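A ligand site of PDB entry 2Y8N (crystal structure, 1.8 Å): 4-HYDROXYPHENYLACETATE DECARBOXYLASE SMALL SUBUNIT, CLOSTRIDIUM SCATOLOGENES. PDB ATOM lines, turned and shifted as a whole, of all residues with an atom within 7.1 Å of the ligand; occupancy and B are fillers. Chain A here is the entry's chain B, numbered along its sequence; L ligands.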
ATOM      1  N   MET A   1      12.679 -14.492  25.278  1.00  0.00           N
ATOM      2  CA  MET A   1      12.486 -13.070  25.505  1.00  0.00           C
ATOM      3  C   MET A   1      12.949 -12.655  26.904  1.00  0.00           C
ATOM      4  O   MET A   1      12.840 -11.486  27.259  1.00  0.00           O
ATOM      5  CB  MET A   1      11.011 -12.686  25.342  1.00  0.00           C
ATOM      6  CG  MET A   1      10.140 -13.077  26.531  1.00  0.00           C
ATOM      7  SD  MET A   1       9.042 -11.771  27.131  1.00  0.00           S
ATOM      8  CE  MET A   1      10.186 -10.555  27.796  1.00  0.00           C
ATOM      9  N   ARG A   2      13.427 -13.619  27.686  1.00  0.00           N
ATOM     10  CA  ARG A   2      14.010 -13.323  29.004  1.00  0.00           C
ATOM     11  C   ARG A   2      15.479 -13.693  29.032  1.00  0.00           C
ATOM     12  O   ARG A   2      15.932 -14.529  28.254  1.00  0.00           O
ATOM     13  CB  ARG A   2      13.294 -14.111  30.097  1.00  0.00           C
ATOM     14  CG  ARG A   2      11.814 -13.830  30.223  1.00  0.00           C
ATOM     15  CD  ARG A   2      11.173 -14.801  31.207  1.00  0.00           C
ATOM     16  NE  ARG A   2      11.212 -16.181  30.735  1.00  0.00           N
ATOM     17  CZ  ARG A   2      11.287 -17.242  31.530  1.00  0.00           C
ATOM     18  NH1 ARG A   2      11.341 -17.082  32.839  1.00  0.00           N
ATOM     19  NH2 ARG A   2      11.312 -18.470  31.005  1.00  0.00           N
ATOM     20  N   HIS A   3      16.230 -13.080  29.944  1.00  0.00           N
ATOM     21  CA  HIS A   3      17.607 -13.492  30.205  1.00  0.00           C
ATOM     22  C   HIS A   3      17.644 -15.000  30.341  1.00  0.00           C
ATOM     23  O   HIS A   3      18.555 -15.660  29.838  1.00  0.00           O
ATOM     24  CB  HIS A   3      18.107 -12.874  31.508  1.00  0.00           C
ATOM     25  CG  HIS A   3      17.831 -11.408  31.640  1.00  0.00           C
ATOM     26  ND1 HIS A   3      18.524 -10.455  30.927  1.00  0.00           N
ATOM     27  CD2 HIS A   3      16.952 -10.735  32.413  1.00  0.00           C
ATOM     28  CE1 HIS A   3      18.071  -9.258  31.243  1.00  0.00           C
ATOM     29  NE2 HIS A   3      17.112  -9.393  32.140  1.00  0.00           N
ATOM     30  N   TYR A   4      16.629 -15.533  31.020  1.00  0.00           N
ATOM     31  CA  TYR A   4      16.547 -16.958  31.306  1.00  0.00           C
ATOM     32  C   TYR A   4      16.552 -17.800  30.036  1.00  0.00           C
ATOM     33  O   TYR A   4      16.924 -18.981  30.062  1.00  0.00           O
ATOM     34  CB  TYR A   4      15.287 -17.243  32.111  1.00  0.00           C
ATOM     35  CG  TYR A   4      15.301 -18.583  32.803  1.00  0.00           C
ATOM     36  CD1 TYR A   4      16.181 -18.823  33.849  1.00  0.00           C
ATOM     37  CD2 TYR A   4      14.416 -19.595  32.426  1.00  0.00           C
ATOM     38  CE1 TYR A   4      16.199 -20.050  34.503  1.00  0.00           C
ATOM     39  CE2 TYR A   4      14.434 -20.822  33.079  1.00  0.00           C
ATOM     40  CZ  TYR A   4      15.326 -21.046  34.111  1.00  0.00           C
ATOM     41  OH  TYR A   4      15.357 -22.255  34.766  1.00  0.00           O
ATOM     42  N   ASP A   5      16.123 -17.208  28.932  1.00  0.00           N
ATOM     43  CA  ASP A   5      16.049 -17.901  27.658  1.00  0.00           C
ATOM     44  C   ASP A   5      17.321 -17.689  26.826  1.00  0.00           C
ATOM     45  O   ASP A   5      17.472 -18.265  25.763  1.00  0.00           O
ATOM     46  CB  ASP A   5      14.833 -17.420  26.860  1.00  0.00           C
ATOM     47  CG  ASP A   5      13.541 -17.501  27.661  1.00  0.00           C
ATOM     48  OD1 ASP A   5      13.067 -18.633  27.908  1.00  0.00           O
ATOM     49  OD2 ASP A   5      12.994 -16.443  28.034  1.00  0.00           O
ATOM     50  N   CYS A   6      18.214 -16.844  27.334  1.00  0.00           N
ATOM     51  CA  CYS A   6      19.401 -16.454  26.583  1.00  0.00           C
ATOM     52  C   CYS A   6      20.596 -17.392  26.797  1.00  0.00           C
ATOM     53  O   CYS A   6      20.809 -17.910  27.888  1.00  0.00           O
ATOM     54  CB  CYS A   6      19.789 -15.011  26.933  1.00  0.00           C
ATOM     55  SG  CYS A   6      21.207 -14.357  26.038  1.00  0.00           S
ATOM     56  N   LYS A   7      21.374 -17.576  25.751  1.00  0.00           N
ATOM     57  CA  LYS A   7      22.580 -18.397  25.803  1.00  0.00           C
ATOM     58  C   LYS A   7      23.633 -17.719  26.677  1.00  0.00           C
ATOM     59  O   LYS A   7      24.550 -18.370  27.193  1.00  0.00           O
ATOM     60  CB  LYS A   7      23.116 -18.623  24.393  1.00  0.00           C
ATOM     61  CG  LYS A   7      24.145 -19.703  24.293  1.00  0.00           C
ATOM     62  CD  LYS A   7      24.579 -19.917  22.864  1.00  0.00           C
ATOM     63  CE  LYS A   7      25.533 -21.094  22.774  1.00  0.00           C
ATOM     64  NZ  LYS A   7      26.249 -21.130  21.464  1.00  0.00           N
ATOM     65  N   ASN A   8      23.504 -16.406  26.841  1.00  0.00           N
ATOM     66  CA  ASN A   8      24.483 -15.658  27.632  1.00  0.00           C
ATOM     67  C   ASN A   8      24.141 -15.659  29.114  1.00  0.00           C
ATOM     68  O   ASN A   8      24.902 -15.155  29.933  1.00  0.00           O
ATOM     69  CB  ASN A   8      24.601 -14.228  27.107  1.00  0.00           C
ATOM     70  CG  ASN A   8      25.149 -14.181  25.689  1.00  0.00           C
ATOM     71  OD1 ASN A   8      25.926 -15.051  25.294  1.00  0.00           O
ATOM     72  ND2 ASN A   8      24.740 -13.171  24.928  1.00  0.00           N
ATOM     73  N   TYR A   9      23.005 -16.232  29.455  1.00  0.00           N
ATOM     74  CA  TYR A   9      22.586 -16.355  30.838  1.00  0.00           C
ATOM     75  C   TYR A   9      23.462 -17.364  31.568  1.00  0.00           C
ATOM     76  O   TYR A   9      23.710 -18.465  31.077  1.00  0.00           O
ATOM     77  CB  TYR A   9      21.139 -16.827  30.863  1.00  0.00           C
ATOM     78  CG  TYR A   9      20.504 -16.920  32.227  1.00  0.00           C
ATOM     79  CD1 TYR A   9      20.105 -15.776  32.900  1.00  0.00           C
ATOM     80  CD2 TYR A   9      20.269 -18.152  32.816  1.00  0.00           C
ATOM     81  CE1 TYR A   9      19.487 -15.857  34.137  1.00  0.00           C
ATOM     82  CE2 TYR A   9      19.654 -18.246  34.055  1.00  0.00           C
ATOM     83  CZ  TYR A   9      19.277 -17.100  34.708  1.00  0.00           C
ATOM     84  OH  TYR A   9      18.663 -17.188  35.934  1.00  0.00           O
ATOM     85  N   ILE A  10      23.946 -16.974  32.751  1.00  0.00           N
ATOM     86  CA  ILE A  10      24.664 -17.887  33.633  1.00  0.00           C
ATOM     87  C   ILE A  10      23.730 -18.253  34.774  1.00  0.00           C
ATOM     88  O   ILE A  10      23.296 -17.372  35.521  1.00  0.00           O
ATOM     89  CB  ILE A  10      25.911 -17.235  34.242  1.00  0.00           C
ATOM     90  CG1 ILE A  10      26.752 -16.504  33.171  1.00  0.00           C
ATOM     91  CG2 ILE A  10      26.739 -18.261  34.991  1.00  0.00           C
ATOM     92  CD1 ILE A  10      27.316 -17.411  32.090  1.00  0.00           C
ATOM     93  N   LEU A  18      23.181 -14.664  36.113  1.00  0.00           N
ATOM     94  CA  LEU A  18      24.052 -13.582  35.708  1.00  0.00           C
ATOM     95  C   LEU A  18      23.932 -13.396  34.216  1.00  0.00           C
ATOM     96  O   LEU A  18      23.612 -14.330  33.483  1.00  0.00           O
ATOM     97  CB  LEU A  18      25.512 -13.910  36.025  1.00  0.00           C
ATOM     98  CG  LEU A  18      25.933 -14.009  37.483  1.00  0.00           C
ATOM     99  CD1 LEU A  18      27.403 -14.383  37.540  1.00  0.00           C
ATOM    100  CD2 LEU A  18      25.661 -12.692  38.213  1.00  0.00           C
ATOM    101  N   CYS A  19      24.193 -12.181  33.755  1.00  0.00           N
ATOM    102  CA  CYS A  19      24.379 -11.985  32.325  1.00  0.00           C
ATOM    103  C   CYS A  19      25.859 -12.119  32.075  1.00  0.00           C
ATOM    104  O   CYS A  19      26.652 -11.424  32.690  1.00  0.00           O
ATOM    105  CB  CYS A  19      23.901 -10.616  31.877  1.00  0.00           C
ATOM    106  SG  CYS A  19      24.601 -10.197  30.277  1.00  0.00           S
ATOM    107  N   ALA A  20      26.230 -13.017  31.156  1.00  0.00           N
ATOM    108  CA  ALA A  20      27.634 -13.232  30.844  1.00  0.00           C
ATOM    109  C   ALA A  20      28.307 -11.945  30.389  1.00  0.00           C
ATOM    110  O   ALA A  20      29.468 -11.694  30.690  1.00  0.00           O
ATOM    111  CB  ALA A  20      27.776 -14.297  29.792  1.00  0.00           C
ATOM    112  N   LEU A  21      27.570 -11.123  29.649  1.00  0.00           N
ATOM    113  CA  LEU A  21      28.140  -9.899  29.092  1.00  0.00           C
ATOM    114  C   LEU A  21      28.367  -8.827  30.170  1.00  0.00           C
ATOM    115  O   LEU A  21      29.481  -8.324  30.339  1.00  0.00           O
ATOM    116  CB  LEU A  21      27.229  -9.350  27.997  1.00  0.00           C
ATOM    117  CG  LEU A  21      26.855 -10.368  26.917  1.00  0.00           C
ATOM    118  CD1 LEU A  21      25.965  -9.716  25.860  1.00  0.00           C
ATOM    119  CD2 LEU A  21      28.101 -10.951  26.284  1.00  0.00           C
ATOM    120  N   THR A  22      27.313  -8.503  30.914  1.00  0.00           N
ATOM    121  CA  THR A  22      27.404  -7.436  31.892  1.00  0.00           C
ATOM    122  C   THR A  22      27.992  -7.950  33.190  1.00  0.00           C
ATOM    123  O   THR A  22      28.523  -7.187  33.991  1.00  0.00           O
ATOM    124  CB  THR A  22      26.011  -6.862  32.193  1.00  0.00           C
ATOM    125  OG1 THR A  22      25.217  -7.857  32.852  1.00  0.00           O
ATOM    126  CG2 THR A  22      25.324  -6.427  30.910  1.00  0.00           C
ATOM    127  N   LYS A  23      27.888  -9.265  33.394  1.00  0.00           N
ATOM    128  CA  LYS A  23      28.294  -9.869  34.648  1.00  0.00           C
ATOM    129  C   LYS A  23      27.428  -9.359  35.792  1.00  0.00           C
ATOM    130  O   LYS A  23      27.754  -9.545  36.961  1.00  0.00           O
ATOM    131  CB  LYS A  23      29.780  -9.621  34.912  1.00  0.00           C
ATOM    132  CG  LYS A  23      30.651 -10.382  33.929  1.00  0.00           C
ATOM    133  CD  LYS A  23      32.046  -9.832  33.859  1.00  0.00           C
ATOM    134  CE  LYS A  23      32.754 -10.323  32.608  1.00  0.00           C
ATOM    135  NZ  LYS A  23      32.032  -9.959  31.351  1.00  0.00           N
ATOM    136  N   GLY A  24      26.301  -8.748  35.430  1.00  0.00           N
ATOM    137  CA  GLY A  24      25.327  -8.302  36.406  1.00  0.00           C
ATOM    138  C   GLY A  24      24.257  -9.349  36.677  1.00  0.00           C
ATOM    139  O   GLY A  24      23.844 -10.094  35.784  1.00  0.00           O
ATOM    140  N   VAL A  26      20.698 -10.914  37.195  1.00  0.00           N
ATOM    141  CA  VAL A  26      19.403 -10.668  36.559  1.00  0.00           C
ATOM    142  C   VAL A  26      18.310 -11.614  37.083  1.00  0.00           C
ATOM    143  O   VAL A  26      18.598 -12.736  37.510  1.00  0.00           O
ATOM    144  CB  VAL A  26      19.495 -10.832  35.022  1.00  0.00           C
ATOM    145  CG1 VAL A  26      20.545  -9.894  34.451  1.00  0.00           C
ATOM    146  CG2 VAL A  26      19.819 -12.281  34.666  1.00  0.00           C
ATOM    147  N   GLY A  32      12.569  -6.461  35.009  1.00  0.00           N
ATOM    148  CA  GLY A  32      13.995  -6.551  34.737  1.00  0.00           C
ATOM    149  C   GLY A  32      14.399  -7.882  34.145  1.00  0.00           C
ATOM    150  O   GLY A  32      15.590  -8.152  33.993  1.00  0.00           O
ATOM    151  N   SER A  33      13.424  -8.716  33.786  1.00  0.00           N
ATOM    152  CA  SER A  33      13.736 -10.053  33.270  1.00  0.00           C
ATOM    153  C   SER A  33      13.760 -10.195  31.738  1.00  0.00           C
ATOM    154  O   SER A  33      14.253 -11.205  31.242  1.00  0.00           O
ATOM    155  CB  SER A  33      12.804 -11.097  33.894  1.00  0.00           C
ATOM    156  OG  SER A  33      11.452 -10.870  33.560  1.00  0.00           O
ATOM    157  N   GLU A  34      13.265  -9.202  31.001  1.00  0.00           N
ATOM    158  CA  GLU A  34      13.220  -9.324  29.545  1.00  0.00           C
ATOM    159  C   GLU A  34      14.596  -9.317  28.897  1.00  0.00           C
ATOM    160  O   GLU A  34      15.521  -8.666  29.368  1.00  0.00           O
ATOM    161  CB  GLU A  34      12.400  -8.223  28.873  1.00  0.00           C
ATOM    162  CG  GLU A  34      11.321  -7.610  29.718  1.00  0.00           C
ATOM    163  CD  GLU A  34      11.839  -6.460  30.559  1.00  0.00           C
ATOM    164  OE1 GLU A  34      13.046  -6.443  30.890  1.00  0.00           O
ATOM    165  OE2 GLU A  34      11.024  -5.577  30.887  1.00  0.00           O
ATOM    166  N   ALA A  35      14.696 -10.041  27.789  1.00  0.00           N
ATOM    167  CA  ALA A  35      15.921 -10.148  27.008  1.00  0.00           C
ATOM    168  C   ALA A  35      16.370  -8.784  26.518  1.00  0.00           C
ATOM    169  O   ALA A  35      15.533  -7.917  26.235  1.00  0.00           O
ATOM    170  CB  ALA A  35      15.696 -11.076  25.835  1.00  0.00           C
ATOM    171  N   CYS A  36      17.677  -8.585  26.409  1.00  0.00           N
ATOM    172  CA  CYS A  36      18.239  -7.380  25.826  1.00  0.00           C
ATOM    173  C   CYS A  36      18.542  -7.621  24.357  1.00  0.00           C
ATOM    174  O   CYS A  36      18.489  -8.758  23.893  1.00  0.00           O
ATOM    175  CB  CYS A  36      19.507  -6.973  26.569  1.00  0.00           C
ATOM    176  SG  CYS A  36      21.039  -7.431  25.728  1.00  0.00           S
ATOM    177  N   PRO A  37      18.859  -6.555  23.597  1.00  0.00           N
ATOM    178  CA  PRO A  37      19.104  -6.682  22.155  1.00  0.00           C
ATOM    179  C   PRO A  37      20.219  -7.672  21.823  1.00  0.00           C
ATOM    180  O   PRO A  37      20.243  -8.216  20.718  1.00  0.00           O
ATOM    181  CB  PRO A  37      19.524  -5.259  21.730  1.00  0.00           C
ATOM    182  CG  PRO A  37      19.738  -4.505  23.015  1.00  0.00           C
ATOM    183  CD  PRO A  37      18.870  -5.146  24.025  1.00  0.00           C
ATOM    184  N   ASN A  38      21.128  -7.893  22.770  1.00  0.00           N
ATOM    185  CA  ASN A  38      22.241  -8.832  22.590  1.00  0.00           C
ATOM    186  C   ASN A  38      21.834 -10.280  22.806  1.00  0.00           C
ATOM    187  O   ASN A  38      22.672 -11.178  22.852  1.00  0.00           O
ATOM    188  CB  ASN A  38      23.404  -8.473  23.522  1.00  0.00           C
ATOM    189  CG  ASN A  38      24.080  -7.170  23.147  1.00  0.00           C
ATOM    190  OD1 ASN A  38      24.297  -6.306  23.995  1.00  0.00           O
ATOM    191  ND2 ASN A  38      24.384  -7.012  21.866  1.00  0.00           N
ATOM    192  N   PHE A  39      20.537 -10.502  22.951  1.00  0.00           N
ATOM    193  CA  PHE A  39      19.980 -11.819  23.202  1.00  0.00           C
ATOM    194  C   PHE A  39      20.375 -12.837  22.132  1.00  0.00           C
ATOM    195  O   PHE A  39      20.326 -12.547  20.935  1.00  0.00           O
ATOM    196  CB  PHE A  39      18.463 -11.740  23.288  1.00  0.00           C
ATOM    197  CG  PHE A  39      17.791 -13.072  23.443  1.00  0.00           C
ATOM    198  CD1 PHE A  39      17.449 -13.824  22.332  1.00  0.00           C
ATOM    199  CD2 PHE A  39      17.482 -13.561  24.702  1.00  0.00           C
ATOM    200  CE1 PHE A  39      16.826 -15.045  22.467  1.00  0.00           C
ATOM    201  CE2 PHE A  39      16.858 -14.788  24.851  1.00  0.00           C
ATOM    202  CZ  PHE A  39      16.526 -15.531  23.736  1.00  0.00           C
ATOM    203  N   LYS A  40      20.760 -14.014  22.595  1.00  0.00           N
ATOM    204  CA  LYS A  40      20.955 -15.192  21.745  1.00  0.00           C
ATOM    205  C   LYS A  40      20.253 -16.369  22.417  1.00  0.00           C
ATOM    206  O   LYS A  40      20.461 -16.625  23.598  1.00  0.00           O
ATOM    207  CB  LYS A  40      22.436 -15.479  21.562  1.00  0.00           C
ATOM    208  CG  LYS A  40      23.142 -14.452  20.697  1.00  0.00           C
ATOM    209  CD  LYS A  40      24.598 -14.301  21.076  1.00  0.00           C
ATOM    210  CE  LYS A  40      25.454 -15.444  20.536  1.00  0.00           C
ATOM    211  NZ  LYS A  40      26.915 -15.207  20.815  1.00  0.00           N
HETATM  212 FE1  LIG L   1      21.149 -12.327  27.432  1.00  0.00          FE
HETATM  213 FE2  LIG L   1      19.962 -10.963  29.453  1.00  0.00          FE
HETATM  214 FE3  LIG L   1      20.948  -9.624  27.302  1.00  0.00          FE
HETATM  215 FE4  LIG L   1      22.620 -10.729  29.112  1.00  0.00          FE
HETATM  216  S1  LIG L   1      21.148  -8.990  29.507  1.00  0.00           S
HETATM  217  S2  LIG L   1      22.818 -10.872  26.827  1.00  0.00           S
HETATM  218  S3  LIG L   1      21.508 -12.665  29.683  1.00  0.00           S
HETATM  219  S4  LIG L   1      19.194 -11.131  27.296  1.00  0.00           S
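ND1 of His 3 is bound to FE2 of the ligand (2.1 Å).
SG of Cys 19 is bound to FE4 of the ligand.
SG of Cys 6 binds FE1 of the ligand, 2.5 Å away.
The backbone NH of Cys 36 lies close to a sulfur (S4) of the ligand (3.1 Å).
An iron atom (FE3) of the ligand is bound by the side-chain sulfur of Cys 36, at 2.7 Å.
ND2 of Asn 8 lies close to S2 of the ligand, 3.5 Å away.
The backbone carbonyl oxygen of Glu 34 sits close to a ring nitrogen (NE2) of His 3 (3.3 Å).
The backbone carbonyl oxygen (O) of Ser 33 lies close to the backbone NH (N) of His 3 (3.0 Å).
O of Gly 32 sits at hydrogen-bond distance from NE2 of His 3 (2.7 Å).
The side-chain sulfur (SG) of Cys 6 lies close to the backbone NH (N) of Asn 8 (3.2 Å).
The side-chain sulfur (SG) of Cys 6 sits close to the backbone carbonyl oxygen (O) of Lys 40, at 3.4 Å.
The side-chain sulfur (SG) of Cys 36 sits close to the backbone NH (N) of Asn 38 (3.0 Å).
The backbone carbonyl oxygen (O) of Met 1 lies within hydrogen-bond range of the backbone NH (N) of Ala 35 (2.4 Å).
O of Asn 8 sits at hydrogen-bond distance from N of Ala 20 (2.8 Å).
Merely in contact with the ligand: Ala 35, Leu 21, Tyr 9, Phe 39 and Asn 38.
Of the 27 residues printed, 10 come within 4 Å of the ligand.
The nearest printed residue that does not touch the ligand is Leu 18 (4.7 Å).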
